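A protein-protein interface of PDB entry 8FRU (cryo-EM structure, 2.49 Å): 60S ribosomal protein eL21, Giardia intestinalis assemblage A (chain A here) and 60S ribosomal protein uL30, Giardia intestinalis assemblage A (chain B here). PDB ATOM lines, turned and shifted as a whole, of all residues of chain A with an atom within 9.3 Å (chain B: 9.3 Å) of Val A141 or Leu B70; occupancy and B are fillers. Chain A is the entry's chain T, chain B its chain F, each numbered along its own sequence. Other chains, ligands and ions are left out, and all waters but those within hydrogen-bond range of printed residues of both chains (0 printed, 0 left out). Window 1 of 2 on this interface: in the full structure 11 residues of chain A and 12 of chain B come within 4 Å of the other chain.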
ATOM      1  N   ALA A 138      -7.548  22.491  -4.820  1.00  0.00           N
ATOM      2  CA  ALA A 138      -6.150  22.090  -4.859  1.00  0.00           C
ATOM      3  C   ALA A 138      -6.015  20.570  -4.928  1.00  0.00           C
ATOM      4  O   ALA A 138      -6.985  19.822  -4.802  1.00  0.00           O
ATOM      5  CB  ALA A 138      -5.405  22.642  -3.639  1.00  0.00           C
ATOM      6  N   ALA A 139      -4.780  20.120  -5.130  1.00  0.00           N
ATOM      7  CA  ALA A 139      -4.495  18.697  -5.249  1.00  0.00           C
ATOM      8  C   ALA A 139      -4.658  17.986  -3.909  1.00  0.00           C
ATOM      9  O   ALA A 139      -4.370  18.539  -2.845  1.00  0.00           O
ATOM     10  CB  ALA A 139      -3.080  18.484  -5.781  1.00  0.00           C
ATOM     11  N   HIS A 140      -5.121  16.741  -3.971  1.00  0.00           N
ATOM     12  CA  HIS A 140      -5.356  15.948  -2.773  1.00  0.00           C
ATOM     13  C   HIS A 140      -5.510  14.489  -3.180  1.00  0.00           C
ATOM     14  O   HIS A 140      -5.588  14.160  -4.364  1.00  0.00           O
ATOM     15  CB  HIS A 140      -6.585  16.447  -2.012  1.00  0.00           C
ATOM     16  CG  HIS A 140      -7.869  16.263  -2.757  1.00  0.00           C
ATOM     17  ND1 HIS A 140      -8.028  16.644  -4.071  1.00  0.00           N
ATOM     18  CD2 HIS A 140      -9.053  15.734  -2.373  1.00  0.00           C
ATOM     19  CE1 HIS A 140      -9.256  16.361  -4.463  1.00  0.00           C
ATOM     20  NE2 HIS A 140      -9.900  15.808  -3.452  1.00  0.00           N
ATOM     21  N   VAL A 141      -5.555  13.615  -2.177  1.00  0.00           N
ATOM     22  CA  VAL A 141      -5.612  12.172  -2.387  1.00  0.00           C
ATOM     23  C   VAL A 141      -6.820  11.614  -1.651  1.00  0.00           C
ATOM     24  O   VAL A 141      -7.060  11.962  -0.492  1.00  0.00           O
ATOM     25  CB  VAL A 141      -4.325  11.473  -1.916  1.00  0.00           C
ATOM     26  CG1 VAL A 141      -4.452   9.976  -2.086  1.00  0.00           C
ATOM     27  CG2 VAL A 141      -3.131  11.993  -2.689  1.00  0.00           C
ATOM     28  N   VAL A 142      -7.573  10.744  -2.322  1.00  0.00           N
ATOM     29  CA  VAL A 142      -8.779  10.150  -1.767  1.00  0.00           C
ATOM     30  C   VAL A 142      -8.628   8.635  -1.758  1.00  0.00           C
ATOM     31  O   VAL A 142      -7.853   8.057  -2.521  1.00  0.00           O
ATOM     32  CB  VAL A 142     -10.042  10.562  -2.550  1.00  0.00           C
ATOM     33  CG1 VAL A 142     -11.287  10.238  -1.762  1.00  0.00           C
ATOM     34  CG2 VAL A 142      -9.999  12.036  -2.882  1.00  0.00           C
ATOM     35  N   SER A 143      -9.381   7.996  -0.871  1.00  0.00           N
ATOM     36  CA  SER A 143      -9.406   6.546  -0.744  1.00  0.00           C
ATOM     37  C   SER A 143     -10.593   5.967  -1.502  1.00  0.00           C
ATOM     38  O   SER A 143     -11.601   6.639  -1.731  1.00  0.00           O
ATOM     39  CB  SER A 143      -9.477   6.134   0.727  1.00  0.00           C
ATOM     40  OG  SER A 143      -9.829   4.772   0.856  1.00  0.00           O
ATOM     41  N   ILE A 144     -10.474   4.697  -1.875  1.00  0.00           N
ATOM     42  CA  ILE A 144     -11.477   4.030  -2.692  1.00  0.00           C
ATOM     43  C   ILE A 144     -12.105   2.893  -1.894  1.00  0.00           C
ATOM     44  O   ILE A 144     -11.418   1.938  -1.508  1.00  0.00           O
ATOM     45  CB  ILE A 144     -10.881   3.502  -4.004  1.00  0.00           C
ATOM     46  CG1 ILE A 144     -10.955   4.573  -5.089  1.00  0.00           C
ATOM     47  CG2 ILE A 144     -11.611   2.252  -4.440  1.00  0.00           C
ATOM     48  CD1 ILE A 144      -9.968   4.363  -6.206  1.00  0.00           C
ATOM     49  N   ALA A 145     -13.409   3.004  -1.649  1.00  0.00           N
ATOM     50  CA  ALA A 145     -14.265   1.909  -1.193  1.00  0.00           C
ATOM     51  C   ALA A 145     -15.564   1.964  -1.988  1.00  0.00           C
ATOM     52  O   ALA A 145     -16.665   1.826  -1.455  1.00  0.00           O
ATOM     53  CB  ALA A 145     -14.529   1.987   0.310  1.00  0.00           C
ATOM     54  N   SER A 146     -15.423   2.165  -3.296  1.00  0.00           N
ATOM     55  CA  SER A 146     -16.488   2.685  -4.136  1.00  0.00           C
ATOM     56  C   SER A 146     -17.619   1.682  -4.320  1.00  0.00           C
ATOM     57  O   SER A 146     -17.460   0.473  -4.143  1.00  0.00           O
ATOM     58  CB  SER A 146     -15.930   3.083  -5.498  1.00  0.00           C
ATOM     59  OG  SER A 146     -14.810   2.289  -5.831  1.00  0.00           O
ATOM     60  N   GLU B  57       4.086  14.733 -11.040  1.00  0.00           N
ATOM     61  CA  GLU B  57       2.698  14.295 -11.129  1.00  0.00           C
ATOM     62  C   GLU B  57       2.613  12.801 -11.416  1.00  0.00           C
ATOM     63  O   GLU B  57       1.807  12.084 -10.803  1.00  0.00           O
ATOM     64  CB  GLU B  57       1.958  15.097 -12.195  1.00  0.00           C
ATOM     65  CG  GLU B  57       0.449  15.068 -12.043  1.00  0.00           C
ATOM     66  CD  GLU B  57      -0.043  16.026 -10.978  1.00  0.00           C
ATOM     67  OE1 GLU B  57       0.469  15.961  -9.840  1.00  0.00           O
ATOM     68  OE2 GLU B  57      -0.932  16.850 -11.279  1.00  0.00           O
ATOM     69  N   LYS B  59       4.829  10.496 -10.632  1.00  0.00           N
ATOM     70  CA  LYS B  59       5.242   9.762  -9.442  1.00  0.00           C
ATOM     71  C   LYS B  59       4.127   9.732  -8.404  1.00  0.00           C
ATOM     72  O   LYS B  59       3.888   8.699  -7.763  1.00  0.00           O
ATOM     73  CB  LYS B  59       6.504  10.387  -8.855  1.00  0.00           C
ATOM     74  CG  LYS B  59       7.160   9.562  -7.772  1.00  0.00           C
ATOM     75  CD  LYS B  59       6.922   8.077  -7.998  1.00  0.00           C
ATOM     76  CE  LYS B  59       7.557   7.240  -6.899  1.00  0.00           C
ATOM     77  NZ  LYS B  59       8.040   5.929  -7.407  1.00  0.00           N
ATOM     78  N   ALA B  60       3.443  10.860  -8.218  1.00  0.00           N
ATOM     79  CA  ALA B  60       2.330  10.897  -7.277  1.00  0.00           C
ATOM     80  C   ALA B  60       1.234   9.928  -7.690  1.00  0.00           C
ATOM     81  O   ALA B  60       0.676   9.212  -6.848  1.00  0.00           O
ATOM     82  CB  ALA B  60       1.777  12.317  -7.172  1.00  0.00           C
ATOM     83  N   ARG B  61       0.911   9.886  -8.984  1.00  0.00           N
ATOM     84  CA  ARG B  61      -0.123   8.963  -9.442  1.00  0.00           C
ATOM     85  C   ARG B  61       0.254   7.522  -9.121  1.00  0.00           C
ATOM     86  O   ARG B  61      -0.566   6.755  -8.606  1.00  0.00           O
ATOM     87  CB  ARG B  61      -0.362   9.136 -10.939  1.00  0.00           C
ATOM     88  N   GLU B  62       1.503   7.142  -9.397  1.00  0.00           N
ATOM     89  CA  GLU B  62       1.914   5.760  -9.147  1.00  0.00           C
ATOM     90  C   GLU B  62       1.872   5.424  -7.659  1.00  0.00           C
ATOM     91  O   GLU B  62       1.317   4.388  -7.250  1.00  0.00           O
ATOM     92  CB  GLU B  62       3.311   5.517  -9.713  1.00  0.00           C
ATOM     93  CG  GLU B  62       3.365   4.403 -10.745  1.00  0.00           C
ATOM     94  CD  GLU B  62       4.689   4.357 -11.484  1.00  0.00           C
ATOM     95  OE1 GLU B  62       5.156   5.423 -11.934  1.00  0.00           O
ATOM     96  OE2 GLU B  62       5.261   3.254 -11.616  1.00  0.00           O
ATOM     97  N   ASN B  63       2.449   6.294  -6.827  1.00  0.00           N
ATOM     98  CA  ASN B  63       2.484   6.015  -5.397  1.00  0.00           C
ATOM     99  C   ASN B  63       1.081   5.911  -4.825  1.00  0.00           C
ATOM    100  O   ASN B  63       0.797   5.016  -4.021  1.00  0.00           O
ATOM    101  CB  ASN B  63       3.278   7.090  -4.661  1.00  0.00           C
ATOM    102  CG  ASN B  63       4.758   7.035  -4.973  1.00  0.00           C
ATOM    103  OD1 ASN B  63       5.341   5.959  -5.087  1.00  0.00           O
ATOM    104  ND2 ASN B  63       5.376   8.201  -5.101  1.00  0.00           N
ATOM    105  N   ALA B  64       0.184   6.816  -5.219  1.00  0.00           N
ATOM    106  CA  ALA B  64      -1.190   6.720  -4.746  1.00  0.00           C
ATOM    107  C   ALA B  64      -1.841   5.433  -5.230  1.00  0.00           C
ATOM    108  O   ALA B  64      -2.590   4.790  -4.489  1.00  0.00           O
ATOM    109  CB  ALA B  64      -1.993   7.938  -5.201  1.00  0.00           C
ATOM    110  N   LEU B  65      -1.556   5.035  -6.472  1.00  0.00           N
ATOM    111  CA  LEU B  65      -2.177   3.838  -7.023  1.00  0.00           C
ATOM    112  C   LEU B  65      -1.796   2.591  -6.243  1.00  0.00           C
ATOM    113  O   LEU B  65      -2.633   1.702  -6.058  1.00  0.00           O
ATOM    114  CB  LEU B  65      -1.785   3.673  -8.488  1.00  0.00           C
ATOM    115  CG  LEU B  65      -2.723   2.823  -9.343  1.00  0.00           C
ATOM    116  CD1 LEU B  65      -2.592   1.354  -8.988  1.00  0.00           C
ATOM    117  CD2 LEU B  65      -4.153   3.305  -9.184  1.00  0.00           C
ATOM    118  N   LYS B  66      -0.545   2.489  -5.790  1.00  0.00           N
ATOM    119  CA  LYS B  66      -0.196   1.286  -5.037  1.00  0.00           C
ATOM    120  C   LYS B  66      -1.028   1.153  -3.763  1.00  0.00           C
ATOM    121  O   LYS B  66      -1.283   0.033  -3.309  1.00  0.00           O
ATOM    122  CB  LYS B  66       1.292   1.259  -4.687  1.00  0.00           C
ATOM    123  CG  LYS B  66       1.706   2.276  -3.645  1.00  0.00           C
ATOM    124  CD  LYS B  66       3.099   1.991  -3.106  1.00  0.00           C
ATOM    125  CE  LYS B  66       4.119   1.862  -4.219  1.00  0.00           C
ATOM    126  NZ  LYS B  66       4.299   3.115  -4.986  1.00  0.00           N
ATOM    127  N   ASN B  67      -1.473   2.269  -3.184  1.00  0.00           N
ATOM    128  CA  ASN B  67      -2.128   2.275  -1.880  1.00  0.00           C
ATOM    129  C   ASN B  67      -3.651   2.315  -1.987  1.00  0.00           C
ATOM    130  O   ASN B  67      -4.325   2.816  -1.082  1.00  0.00           O
ATOM    131  CB  ASN B  67      -1.615   3.455  -1.054  1.00  0.00           C
ATOM    132  CG  ASN B  67      -1.851   3.281   0.433  1.00  0.00           C
ATOM    133  OD1 ASN B  67      -0.953   3.472   1.249  1.00  0.00           O
ATOM    134  ND2 ASN B  67      -3.076   2.928   0.793  1.00  0.00           N
ATOM    135  N   ASN B  68      -4.212   1.795  -3.077  1.00  0.00           N
ATOM    136  CA  ASN B  68      -5.660   1.761  -3.265  1.00  0.00           C
ATOM    137  C   ASN B  68      -6.277   3.145  -3.065  1.00  0.00           C
ATOM    138  O   ASN B  68      -7.277   3.318  -2.366  1.00  0.00           O
ATOM    139  CB  ASN B  68      -6.303   0.739  -2.330  1.00  0.00           C
ATOM    140  CG  ASN B  68      -7.736   0.440  -2.698  1.00  0.00           C
ATOM    141  N   GLN B  69      -5.672   4.140  -3.701  1.00  0.00           N
ATOM    142  CA  GLN B  69      -6.091   5.518  -3.535  1.00  0.00           C
ATOM    143  C   GLN B  69      -6.096   6.201  -4.892  1.00  0.00           C
ATOM    144  O   GLN B  69      -5.425   5.765  -5.829  1.00  0.00           O
ATOM    145  CB  GLN B  69      -5.172   6.255  -2.560  1.00  0.00           C
ATOM    146  CG  GLN B  69      -5.548   6.051  -1.112  1.00  0.00           C
ATOM    147  CD  GLN B  69      -4.768   6.943  -0.177  1.00  0.00           C
ATOM    148  OE1 GLN B  69      -3.540   6.967  -0.207  1.00  0.00           O
ATOM    149  NE2 GLN B  69      -5.479   7.686   0.659  1.00  0.00           N
ATOM    150  N   LEU B  70      -6.877   7.268  -4.998  1.00  0.00           N
ATOM    151  CA  LEU B  70      -6.930   8.076  -6.206  1.00  0.00           C
ATOM    152  C   LEU B  70      -6.241   9.409  -5.970  1.00  0.00           C
ATOM    153  O   LEU B  70      -6.446  10.051  -4.938  1.00  0.00           O
ATOM    154  CB  LEU B  70      -8.369   8.313  -6.655  1.00  0.00           C
ATOM    155  CG  LEU B  70      -8.937   7.292  -7.636  1.00  0.00           C
ATOM    156  CD1 LEU B  70     -10.388   7.599  -7.935  1.00  0.00           C
ATOM    157  CD2 LEU B  70      -8.116   7.275  -8.902  1.00  0.00           C
ATOM    158  N   TYR B  71      -5.418   9.814  -6.928  1.00  0.00           N
ATOM    159  CA  TYR B  71      -4.768  11.115  -6.896  1.00  0.00           C
ATOM    160  C   TYR B  71      -5.570  12.095  -7.745  1.00  0.00           C
ATOM    161  O   TYR B  71      -5.728  11.891  -8.952  1.00  0.00           O
ATOM    162  CB  TYR B  71      -3.333  11.005  -7.401  1.00  0.00           C
ATOM    163  CG  TYR B  71      -2.623  12.325  -7.489  1.00  0.00           C
ATOM    164  CD1 TYR B  71      -2.205  12.988  -6.348  1.00  0.00           C
ATOM    165  CD2 TYR B  71      -2.373  12.912  -8.716  1.00  0.00           C
ATOM    166  CE1 TYR B  71      -1.559  14.197  -6.429  1.00  0.00           C
ATOM    167  CE2 TYR B  71      -1.729  14.121  -8.806  1.00  0.00           C
ATOM    168  CZ  TYR B  71      -1.323  14.759  -7.662  1.00  0.00           C
ATOM    169  OH  TYR B  71      -0.678  15.966  -7.753  1.00  0.00           O
ATOM    170  N   VAL B  72      -6.082  13.150  -7.118  1.00  0.00           N
ATOM    171  CA  VAL B  72      -6.867  14.170  -7.807  1.00  0.00           C
ATOM    172  C   VAL B  72      -5.961  15.376  -8.040  1.00  0.00           C
ATOM    173  O   VAL B  72      -5.549  16.024  -7.066  1.00  0.00           O
ATOM    174  CB  VAL B  72      -8.116  14.557  -7.006  1.00  0.00           C
ATOM    175  CG1 VAL B  72      -9.032  15.417  -7.848  1.00  0.00           C
ATOM    176  CG2 VAL B  72      -8.841  13.319  -6.536  1.00  0.00           C
ATOM    177  N   PRO B  73      -5.625  15.706  -9.280  1.00  0.00           N
ATOM    178  CA  PRO B  73      -4.720  16.829  -9.546  1.00  0.00           C
ATOM    179  C   PRO B  73      -5.433  18.172  -9.408  1.00  0.00           C
ATOM    180  O   PRO B  73      -6.635  18.255  -9.182  1.00  0.00           O
ATOM    181  CB  PRO B  73      -4.265  16.579 -10.985  1.00  0.00           C
ATOM    182  CG  PRO B  73      -5.362  15.809 -11.601  1.00  0.00           C
ATOM    183  CD  PRO B  73      -6.024  15.009 -10.513  1.00  0.00           C
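O of His A140 is in hydrogen-bond range of N of Val B72 (3.0 Å).
The backbone NH of Leu B70 sits at hydrogen-bond distance from the backbone carbonyl oxygen of Val A142 (2.8 Å).
O of Ala A138 lies within hydrogen-bond range of ND1 of His A140, 3.4 Å away.
The backbone NH of Gln B69 is in hydrogen-bond range of the backbone carbonyl oxygen of Ala B64 (3.2 Å).
Among the printed residues, pairs that only touch across the chains: Ala A139 with Tyr B71 (3.9998 Å), Ala A139 with Val B72 (3.4 Å), His A140 with Tyr B71 (3.96 Å), Val A141 with Gln B69 (3.6 Å), Val A141 with Leu B70 (3.4 Å), Val A141 with Tyr B71 (3.9 Å), Val A142 with Gln B69 (3.2 Å), Ser A143 with Gln B69 (3.9 Å), Ile A144 with Asn B68 (3.5 Å) and Ile A144 with Leu B70 (3.4 Å).
Val A141 touches three residues of chain B.
Leu B70 touches just these residues of chain A: Val A141 (3.4 Å), Val A142 (2.8 Å) and Ile A144 (3.4 Å).
Of chain B, only Gln B69 (3.2 Å) and Leu B70 (2.8 Å) come within 4 Å of Val A142.
Gln B69 touches just these residues of chain A: Val A141, Val A142 and Ser A143.
Of the printed residues of chain B, Ile A144 touches Asn B68 and Leu B70.
Printed residues of chain A within 4 Å of Tyr B71: Ala A139, His A140 and Val A141.
Printed residues of chain B within 4 Å of Ala A139: Tyr B71 and Val B72.
Ser A146 touches none of the printed residues of chain B.
Asn B63 touches none of the printed residues of chain A.
The nearest residue of chain B that does not touch Val A141 is Ala B64 (4.5 Å).
The nearest residue of chain A that does not touch Leu B70 is His A140 (4.2 Å).
The nearest printed residue of chain B that does not touch Ala A139 is Pro B73 (4.3 Å).
Of the 9 printed residues of chain A, 6 touch a printed residue of chain B.
Hydrophobic or aromatic side chains of chain A that line the printed part of chain B: Ala A139, His A140, Val A141 and Ile A144.
Hydrophobic or aromatic side chains of chain B that line the printed part of chain A: Leu B70, Tyr B71 and Val B72.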
